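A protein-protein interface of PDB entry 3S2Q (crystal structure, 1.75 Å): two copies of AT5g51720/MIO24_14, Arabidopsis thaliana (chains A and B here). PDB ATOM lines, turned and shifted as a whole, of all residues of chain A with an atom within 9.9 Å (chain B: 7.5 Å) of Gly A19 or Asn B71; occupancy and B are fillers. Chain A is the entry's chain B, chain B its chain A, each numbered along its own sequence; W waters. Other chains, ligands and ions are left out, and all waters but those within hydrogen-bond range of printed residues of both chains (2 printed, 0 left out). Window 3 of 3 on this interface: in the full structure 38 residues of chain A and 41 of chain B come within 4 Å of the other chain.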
ATOM      1  N   GLY A  19       1.469  13.585 -17.248  1.00  0.00           N
ATOM      2  CA  GLY A  19       0.470  14.568 -16.769  1.00  0.00           C
ATOM      3  C   GLY A  19       0.522  15.878 -17.549  1.00  0.00           C
ATOM      4  O   GLY A  19       1.241  16.820 -17.175  1.00  0.00           O
ATOM      5  N   GLY A  20      -0.251  15.942 -18.625  1.00  0.00           N
ATOM      6  CA  GLY A  20      -0.500  17.215 -19.300  1.00  0.00           C
ATOM      7  C   GLY A  20      -1.291  18.097 -18.338  1.00  0.00           C
ATOM      8  O   GLY A  20      -1.915  17.596 -17.387  1.00  0.00           O
ATOM      9  N   ILE A  21      -1.254  19.411 -18.550  1.00  0.00           N
ATOM     10  CA  ILE A  21      -1.904  20.323 -17.594  1.00  0.00           C
ATOM     11  C   ILE A  21      -3.159  20.981 -18.181  1.00  0.00           C
ATOM     12  O   ILE A  21      -3.965  21.590 -17.459  1.00  0.00           O
ATOM     13  CB  ILE A  21      -0.923  21.380 -17.044  1.00  0.00           C
ATOM     14  CG1 ILE A  21      -0.674  22.482 -18.060  1.00  0.00           C
ATOM     15  CG2 ILE A  21       0.423  20.736 -16.603  1.00  0.00           C
ATOM     16  CD1 ILE A  21       0.309  23.543 -17.595  1.00  0.00           C
ATOM     17  N   ASN A  22      -3.327  20.855 -19.487  1.00  0.00           N
ATOM     18  CA  ASN A  22      -4.425  21.527 -20.180  1.00  0.00           C
ATOM     19  C   ASN A  22      -5.417  20.518 -20.736  1.00  0.00           C
ATOM     20  O   ASN A  22      -5.166  19.957 -21.794  1.00  0.00           O
ATOM     21  CB  ASN A  22      -3.880  22.402 -21.333  1.00  0.00           C
ATOM     22  CG  ASN A  22      -5.002  22.960 -22.228  1.00  0.00           C
ATOM     23  OD1 ASN A  22      -6.146  23.143 -21.772  1.00  0.00           O
ATOM     24  ND2 ASN A  22      -4.685  23.213 -23.510  1.00  0.00           N
ATOM     25  N   PRO A  23      -6.553  20.306 -20.052  1.00  0.00           N
ATOM     26  CA  PRO A  23      -7.501  19.306 -20.523  1.00  0.00           C
ATOM     27  C   PRO A  23      -8.083  19.573 -21.925  1.00  0.00           C
ATOM     28  O   PRO A  23      -8.197  18.639 -22.718  1.00  0.00           O
ATOM     29  CB  PRO A  23      -8.600  19.317 -19.452  1.00  0.00           C
ATOM     30  CG  PRO A  23      -7.932  19.836 -18.214  1.00  0.00           C
ATOM     31  CD  PRO A  23      -6.997  20.908 -18.781  1.00  0.00           C
ATOM     32  N   LYS A  27      -6.989  22.623 -28.376  1.00  0.00           N
ATOM     33  CA  LYS A  27      -6.247  21.409 -28.758  1.00  0.00           C
ATOM     34  C   LYS A  27      -6.020  21.348 -30.277  1.00  0.00           C
ATOM     35  O   LYS A  27      -5.233  20.534 -30.758  1.00  0.00           O
ATOM     36  CB  LYS A  27      -6.961  20.164 -28.208  1.00  0.00           C
ATOM     37  CG  LYS A  27      -6.933  20.065 -26.695  1.00  0.00           C
ATOM     38  CD  LYS A  27      -5.467  20.043 -26.214  1.00  0.00           C
ATOM     39  CE  LYS A  27      -5.360  19.886 -24.732  1.00  0.00           C
ATOM     40  NZ  LYS A  27      -3.922  19.781 -24.261  1.00  0.00           N
ATOM     41  N   ARG A  53      -8.194  26.331 -16.911  1.00  0.00           N
ATOM     42  CA  ARG A  53      -9.594  25.942 -16.642  1.00  0.00           C
ATOM     43  C   ARG A  53     -10.576  27.085 -16.923  1.00  0.00           C
ATOM     44  O   ARG A  53     -11.800  26.857 -16.927  1.00  0.00           O
ATOM     45  CB  ARG A  53      -9.802  25.501 -15.170  1.00  0.00           C
ATOM     46  CG  ARG A  53      -8.869  24.408 -14.582  1.00  0.00           C
ATOM     47  CD  ARG A  53      -8.763  23.290 -15.522  1.00  0.00           C
ATOM     48  NE  ARG A  53      -8.214  22.012 -15.024  1.00  0.00           N
ATOM     49  CZ  ARG A  53      -6.970  21.590 -15.218  1.00  0.00           C
ATOM     50  NH1 ARG A  53      -6.076  22.382 -15.798  1.00  0.00           N
ATOM     51  NH2 ARG A  53      -6.617  20.361 -14.830  1.00  0.00           N
ATOM     52  N   GLY B  20      -3.378  17.853  -9.950  1.00  0.00           N
ATOM     53  CA  GLY B  20      -2.735  19.153  -9.822  1.00  0.00           C
ATOM     54  C   GLY B  20      -1.805  19.419 -10.976  1.00  0.00           C
ATOM     55  O   GLY B  20      -1.330  18.491 -11.661  1.00  0.00           O
ATOM     56  N   ILE B  21      -1.512  20.690 -11.197  1.00  0.00           N
ATOM     57  CA  ILE B  21      -0.709  21.064 -12.354  1.00  0.00           C
ATOM     58  C   ILE B  21       0.622  21.692 -11.959  1.00  0.00           C
ATOM     59  O   ILE B  21       1.486  21.858 -12.811  1.00  0.00           O
ATOM     60  CB  ILE B  21      -1.474  22.002 -13.330  1.00  0.00           C
ATOM     61  CG1 ILE B  21      -1.718  23.387 -12.695  1.00  0.00           C
ATOM     62  CG2 ILE B  21      -2.764  21.336 -13.796  1.00  0.00           C
ATOM     63  CD1 ILE B  21      -2.204  24.450 -13.714  1.00  0.00           C
ATOM     64  N   ARG B  53       6.478  25.012 -15.000  1.00  0.00           N
ATOM     65  CA  ARG B  53       7.747  24.267 -15.090  1.00  0.00           C
ATOM     66  C   ARG B  53       8.962  25.148 -15.239  1.00  0.00           C
ATOM     67  O   ARG B  53      10.086  24.637 -15.283  1.00  0.00           O
ATOM     68  CB  ARG B  53       7.719  23.229 -16.226  1.00  0.00           C
ATOM     69  CG  ARG B  53       6.531  22.218 -16.201  1.00  0.00           C
ATOM     70  CD  ARG B  53       6.551  21.374 -14.972  1.00  0.00           C
ATOM     71  NE  ARG B  53       5.562  20.281 -14.970  1.00  0.00           N
ATOM     72  CZ  ARG B  53       4.281  20.411 -14.608  1.00  0.00           C
ATOM     73  NH1 ARG B  53       3.799  21.594 -14.215  1.00  0.00           N
ATOM     74  NH2 ARG B  53       3.482  19.353 -14.598  1.00  0.00           N
ATOM     75  N   HIS B  64       8.294  24.786 -21.233  1.00  0.00           N
ATOM     76  CA  HIS B  64       7.039  24.277 -21.775  1.00  0.00           C
ATOM     77  C   HIS B  64       7.263  23.294 -22.955  1.00  0.00           C
ATOM     78  O   HIS B  64       6.468  22.371 -23.174  1.00  0.00           O
ATOM     79  CB  HIS B  64       6.114  25.444 -22.186  1.00  0.00           C
ATOM     80  CG  HIS B  64       6.727  26.395 -23.178  1.00  0.00           C
ATOM     81  ND1 HIS B  64       7.447  27.511 -22.799  1.00  0.00           N
ATOM     82  CD2 HIS B  64       6.722  26.392 -24.533  1.00  0.00           C
ATOM     83  CE1 HIS B  64       7.845  28.165 -23.882  1.00  0.00           C
ATOM     84  NE2 HIS B  64       7.415  27.509 -24.947  1.00  0.00           N
ATOM     85  N   VAL B  65       8.356  23.469 -23.688  1.00  0.00           N
ATOM     86  CA  VAL B  65       8.571  22.654 -24.886  1.00  0.00           C
ATOM     87  C   VAL B  65       8.800  21.184 -24.476  1.00  0.00           C
ATOM     88  O   VAL B  65       8.136  20.262 -24.990  1.00  0.00           O
ATOM     89  CB  VAL B  65       9.757  23.191 -25.760  1.00  0.00           C
ATOM     90  CG1 VAL B  65      10.029  22.244 -26.939  1.00  0.00           C
ATOM     91  CG2 VAL B  65       9.444  24.590 -26.303  1.00  0.00           C
ATOM     92  N   LYS B  66       9.739  20.992 -23.547  1.00  0.00           N
ATOM     93  CA  LYS B  66      10.072  19.656 -23.000  1.00  0.00           C
ATOM     94  C   LYS B  66       8.851  19.024 -22.322  1.00  0.00           C
ATOM     95  O   LYS B  66       8.568  17.846 -22.520  1.00  0.00           O
ATOM     96  CB  LYS B  66      11.260  19.805 -22.031  1.00  0.00           C
ATOM     97  CG  LYS B  66      11.730  18.552 -21.278  1.00  0.00           C
ATOM     98  CD  LYS B  66      12.624  19.061 -20.131  1.00  0.00           C
ATOM     99  CE  LYS B  66      13.038  17.984 -19.129  1.00  0.00           C
ATOM    100  NZ  LYS B  66      14.468  17.529 -19.327  1.00  0.00           N
ATOM    101  N   HIS B  67       8.109  19.829 -21.558  1.00  0.00           N
ATOM    102  CA  HIS B  67       6.855  19.387 -20.950  1.00  0.00           C
ATOM    103  C   HIS B  67       5.851  18.896 -21.995  1.00  0.00           C
ATOM    104  O   HIS B  67       5.226  17.843 -21.816  1.00  0.00           O
ATOM    105  CB  HIS B  67       6.203  20.526 -20.124  1.00  0.00           C
ATOM    106  CG  HIS B  67       4.768  20.248 -19.796  1.00  0.00           C
ATOM    107  ND1 HIS B  67       4.396  19.401 -18.772  1.00  0.00           N
ATOM    108  CD2 HIS B  67       3.618  20.628 -20.408  1.00  0.00           C
ATOM    109  CE1 HIS B  67       3.077  19.308 -18.739  1.00  0.00           C
ATOM    110  NE2 HIS B  67       2.584  20.024 -19.732  1.00  0.00           N
ATOM    111  N   ASN B  68       5.661  19.668 -23.068  1.00  0.00           N
ATOM    112  CA  ASN B  68       4.663  19.321 -24.073  1.00  0.00           C
ATOM    113  C   ASN B  68       5.011  17.997 -24.749  1.00  0.00           C
ATOM    114  O   ASN B  68       4.135  17.166 -24.971  1.00  0.00           O
ATOM    115  CB  ASN B  68       4.541  20.404 -25.142  1.00  0.00           C
ATOM    116  CG  ASN B  68       3.744  21.590 -24.668  1.00  0.00           C
ATOM    117  OD1 ASN B  68       2.964  21.475 -23.712  1.00  0.00           O
ATOM    118  ND2 ASN B  68       3.946  22.753 -25.319  1.00  0.00           N
ATOM    119  N   LYS B  69       6.292  17.849 -25.084  1.00  0.00           N
ATOM    120  CA  LYS B  69       6.820  16.616 -25.699  1.00  0.00           C
ATOM    121  C   LYS B  69       6.629  15.407 -24.785  1.00  0.00           C
ATOM    122  O   LYS B  69       6.164  14.355 -25.230  1.00  0.00           O
ATOM    123  CB  LYS B  69       8.307  16.793 -26.055  1.00  0.00           C
ATOM    124  CG  LYS B  69       8.973  15.590 -26.786  1.00  0.00           C
ATOM    125  CD  LYS B  69       8.341  15.292 -28.152  1.00  0.00           C
ATOM    126  CE  LYS B  69       9.012  14.060 -28.819  1.00  0.00           C
ATOM    127  NZ  LYS B  69       8.342  13.568 -30.102  1.00  0.00           N
ATOM    128  N   ALA B  70       6.964  15.550 -23.509  1.00  0.00           N
ATOM    129  CA  ALA B  70       6.899  14.413 -22.577  1.00  0.00           C
ATOM    130  C   ALA B  70       5.470  13.970 -22.243  1.00  0.00           C
ATOM    131  O   ALA B  70       5.222  12.788 -21.921  1.00  0.00           O
ATOM    132  CB  ALA B  70       7.688  14.718 -21.298  1.00  0.00           C
ATOM    133  N   ASN B  71       4.529  14.906 -22.345  1.00  0.00           N
ATOM    134  CA  ASN B  71       3.187  14.689 -21.826  1.00  0.00           C
ATOM    135  C   ASN B  71       2.092  14.753 -22.859  1.00  0.00           C
ATOM    136  O   ASN B  71       0.908  14.602 -22.515  1.00  0.00           O
ATOM    137  CB  ASN B  71       2.920  15.667 -20.675  1.00  0.00           C
ATOM    138  CG  ASN B  71       3.808  15.388 -19.499  1.00  0.00           C
ATOM    139  OD1 ASN B  71       3.640  14.361 -18.818  1.00  0.00           O
ATOM    140  ND2 ASN B  71       4.782  16.271 -19.257  1.00  0.00           N
ATOM    141  N   GLY B  72       2.485  14.954 -24.117  1.00  0.00           N
ATOM    142  CA  GLY B  72       1.540  15.109 -25.223  1.00  0.00           C
ATOM    143  C   GLY B  72       0.603  16.280 -24.930  1.00  0.00           C
ATOM    144  O   GLY B  72      -0.607  16.184 -25.151  1.00  0.00           O
ATOM    145  N   ASP B  73       1.179  17.387 -24.455  1.00  0.00           N
ATOM    146  CA  ASP B  73       0.390  18.565 -24.059  1.00  0.00           C
ATOM    147  C   ASP B  73       0.658  19.684 -25.086  1.00  0.00           C
ATOM    148  O   ASP B  73       1.467  19.488 -26.010  1.00  0.00           O
ATOM    149  CB  ASP B  73       0.815  18.995 -22.657  1.00  0.00           C
ATOM    150  CG  ASP B  73      -0.286  19.750 -21.878  1.00  0.00           C
ATOM    151  OD1 ASP B  73      -1.430  19.955 -22.369  1.00  0.00           O
ATOM    152  OD2 ASP B  73       0.020  20.140 -20.730  1.00  0.00           O
ATOM    153  N   ASN B  74      -0.012  20.835 -24.943  1.00  0.00           N
ATOM    154  CA  ASN B  74       0.104  21.920 -25.952  1.00  0.00           C
ATOM    155  C   ASN B  74       0.122  23.321 -25.307  1.00  0.00           C
ATOM    156  O   ASN B  74      -0.419  24.271 -25.873  1.00  0.00           O
ATOM    157  CB  ASN B  74      -1.046  21.851 -26.973  1.00  0.00           C
ATOM    158  CG  ASN B  74      -2.383  22.237 -26.367  1.00  0.00           C
ATOM    159  OD1 ASN B  74      -2.599  22.041 -25.173  1.00  0.00           O
ATOM    160  ND2 ASN B  74      -3.300  22.783 -27.188  1.00  0.00           N
HETATM  161  O   HOH W   1      -2.940  17.823 -22.205  1.00  0.00           O
HETATM  162  O   HOH W   2      -2.416  18.198 -25.972  1.00  0.00           O
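The backbone NH (N) of Gly A19 sits at hydrogen-bond distance from the side-chain amide oxygen (OD1) of Asn B71. N of Ile A21 sits at hydrogen-bond distance from OD2 of Asp B73. OD1 of Asp B73 lies within salt-bridge range of NZ of Lys A27 (3.1 Å). The side-chain amide oxygen (OD1) of Asn B74 sits at hydrogen-bond distance from the side-chain amide nitrogen (ND2) of Asn A22, 2.9 Å away. OD1 of Asn B74 is in hydrogen-bond range of NZ of Lys A27 (2.8 Å).
O of His B67 lies within hydrogen-bond range of ND2 of Asn B71 (3.0 Å). OD2 of Asp B73 sits at hydrogen-bond distance from NE2 of His B67, 2.8 Å away. The backbone carbonyl oxygen of Asn B68 sits at hydrogen-bond distance from the backbone NH of Asp B73, at 3.0 Å. The backbone NH (N) of Asn B74 is in hydrogen-bond range of the side-chain amide oxygen (OD1) of Asn B68 (3.3 Å). The backbone carbonyl oxygen of Ile A21 lies within hydrogen-bond range of the guanidinium group of Arg A53 (2.8 Å). The side-chain amino group (NZ) of Lys A27 lies within hydrogen-bond range of the backbone carbonyl oxygen (O) of Asn A22 (2.8 Å).
His B67 touches Gly A19. Asn B71 touches Gly A20. Asp B73 touches Gly A20 (OD2 to CA, 3.3 Å). CB of Ile A21 touches CG2 of Ile B21 (3.7 Å). CG2 of Ile A21 touches NH2 of Arg B53, at 3.9 Å. Ile A21 touches His B67 (CG2 to CE1, 3.7 Å). N of Asn A22 touches OD1 of Asp B73, 3.6 Å away.
Gly A19 touches two residues of chain B. Asn B71 touches just these residues of chain A: Gly A19 (2.8 Å) and Gly A20 (3.8 Å). No residue of chain A comes within 4 Å of Ala B70. No residue of chain A comes within 4 Å of Gly B72. Of chain A, only Gly A20, Ile A21, Asn A22 and Lys A27 come within 4 Å of Asp B73. Of the printed residues of chain B, Ile A21 touches Ile B21, Arg B53, His B67 and Asp B73. Of the printed residues of chain A, Asn B74 touches Asn A22 and Lys A27. The nearest residue of chain B that does not touch Gly A19 is Arg B53 (4.3 Å). The nearest residue of chain A that does not touch Asn B71 is Ile A21 (6.0 Å). The nearest printed residue of chain A that does not touch Ile B21 is Arg A53 (4.01 Å).
Printed residues of chain A that touch a printed residue of chain B: Gly A19, Gly A20, Ile A21, Asn A22 and Lys A27. Hydrophobic or aromatic side chains of chain A that line the printed part of chain B: Ile A21. Of the 14 printed residues of chain B, 6 touch a printed residue of chain A. Hydrophobic or aromatic side chains of chain B within 4 Å of the printed part of chain A: Ile B21 and His B67. Among the printed residues, 12 pairs touch across the chains. Among the printed residues, Asp or Glu carboxylates within 4 Å of a Lys or Arg side-chain nitrogen of the other chain: Lys A27 with Asp B73.
Ile A21 touches its own counterpart, Ile B21. Ile A21 touches Arg B53, but with the chains exchanged Arg A53 does not touch Ile B21 (4.01 Å). Of the 12 pairs that touch across the chains among the printed residues, 1 has its exchanged pair printed and touching as well.
Water W1 lies within hydrogen-bond range of OD1 of Asp B73 (2.6 Å), NZ of Lys A27 (3.0 Å) and O of Asn A22 (3.1 Å). Water W2 bridges the side-chain amino group of Lys A27 (2.8 Å) and the backbone carbonyl oxygen of Gly B72 (2.8 Å).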
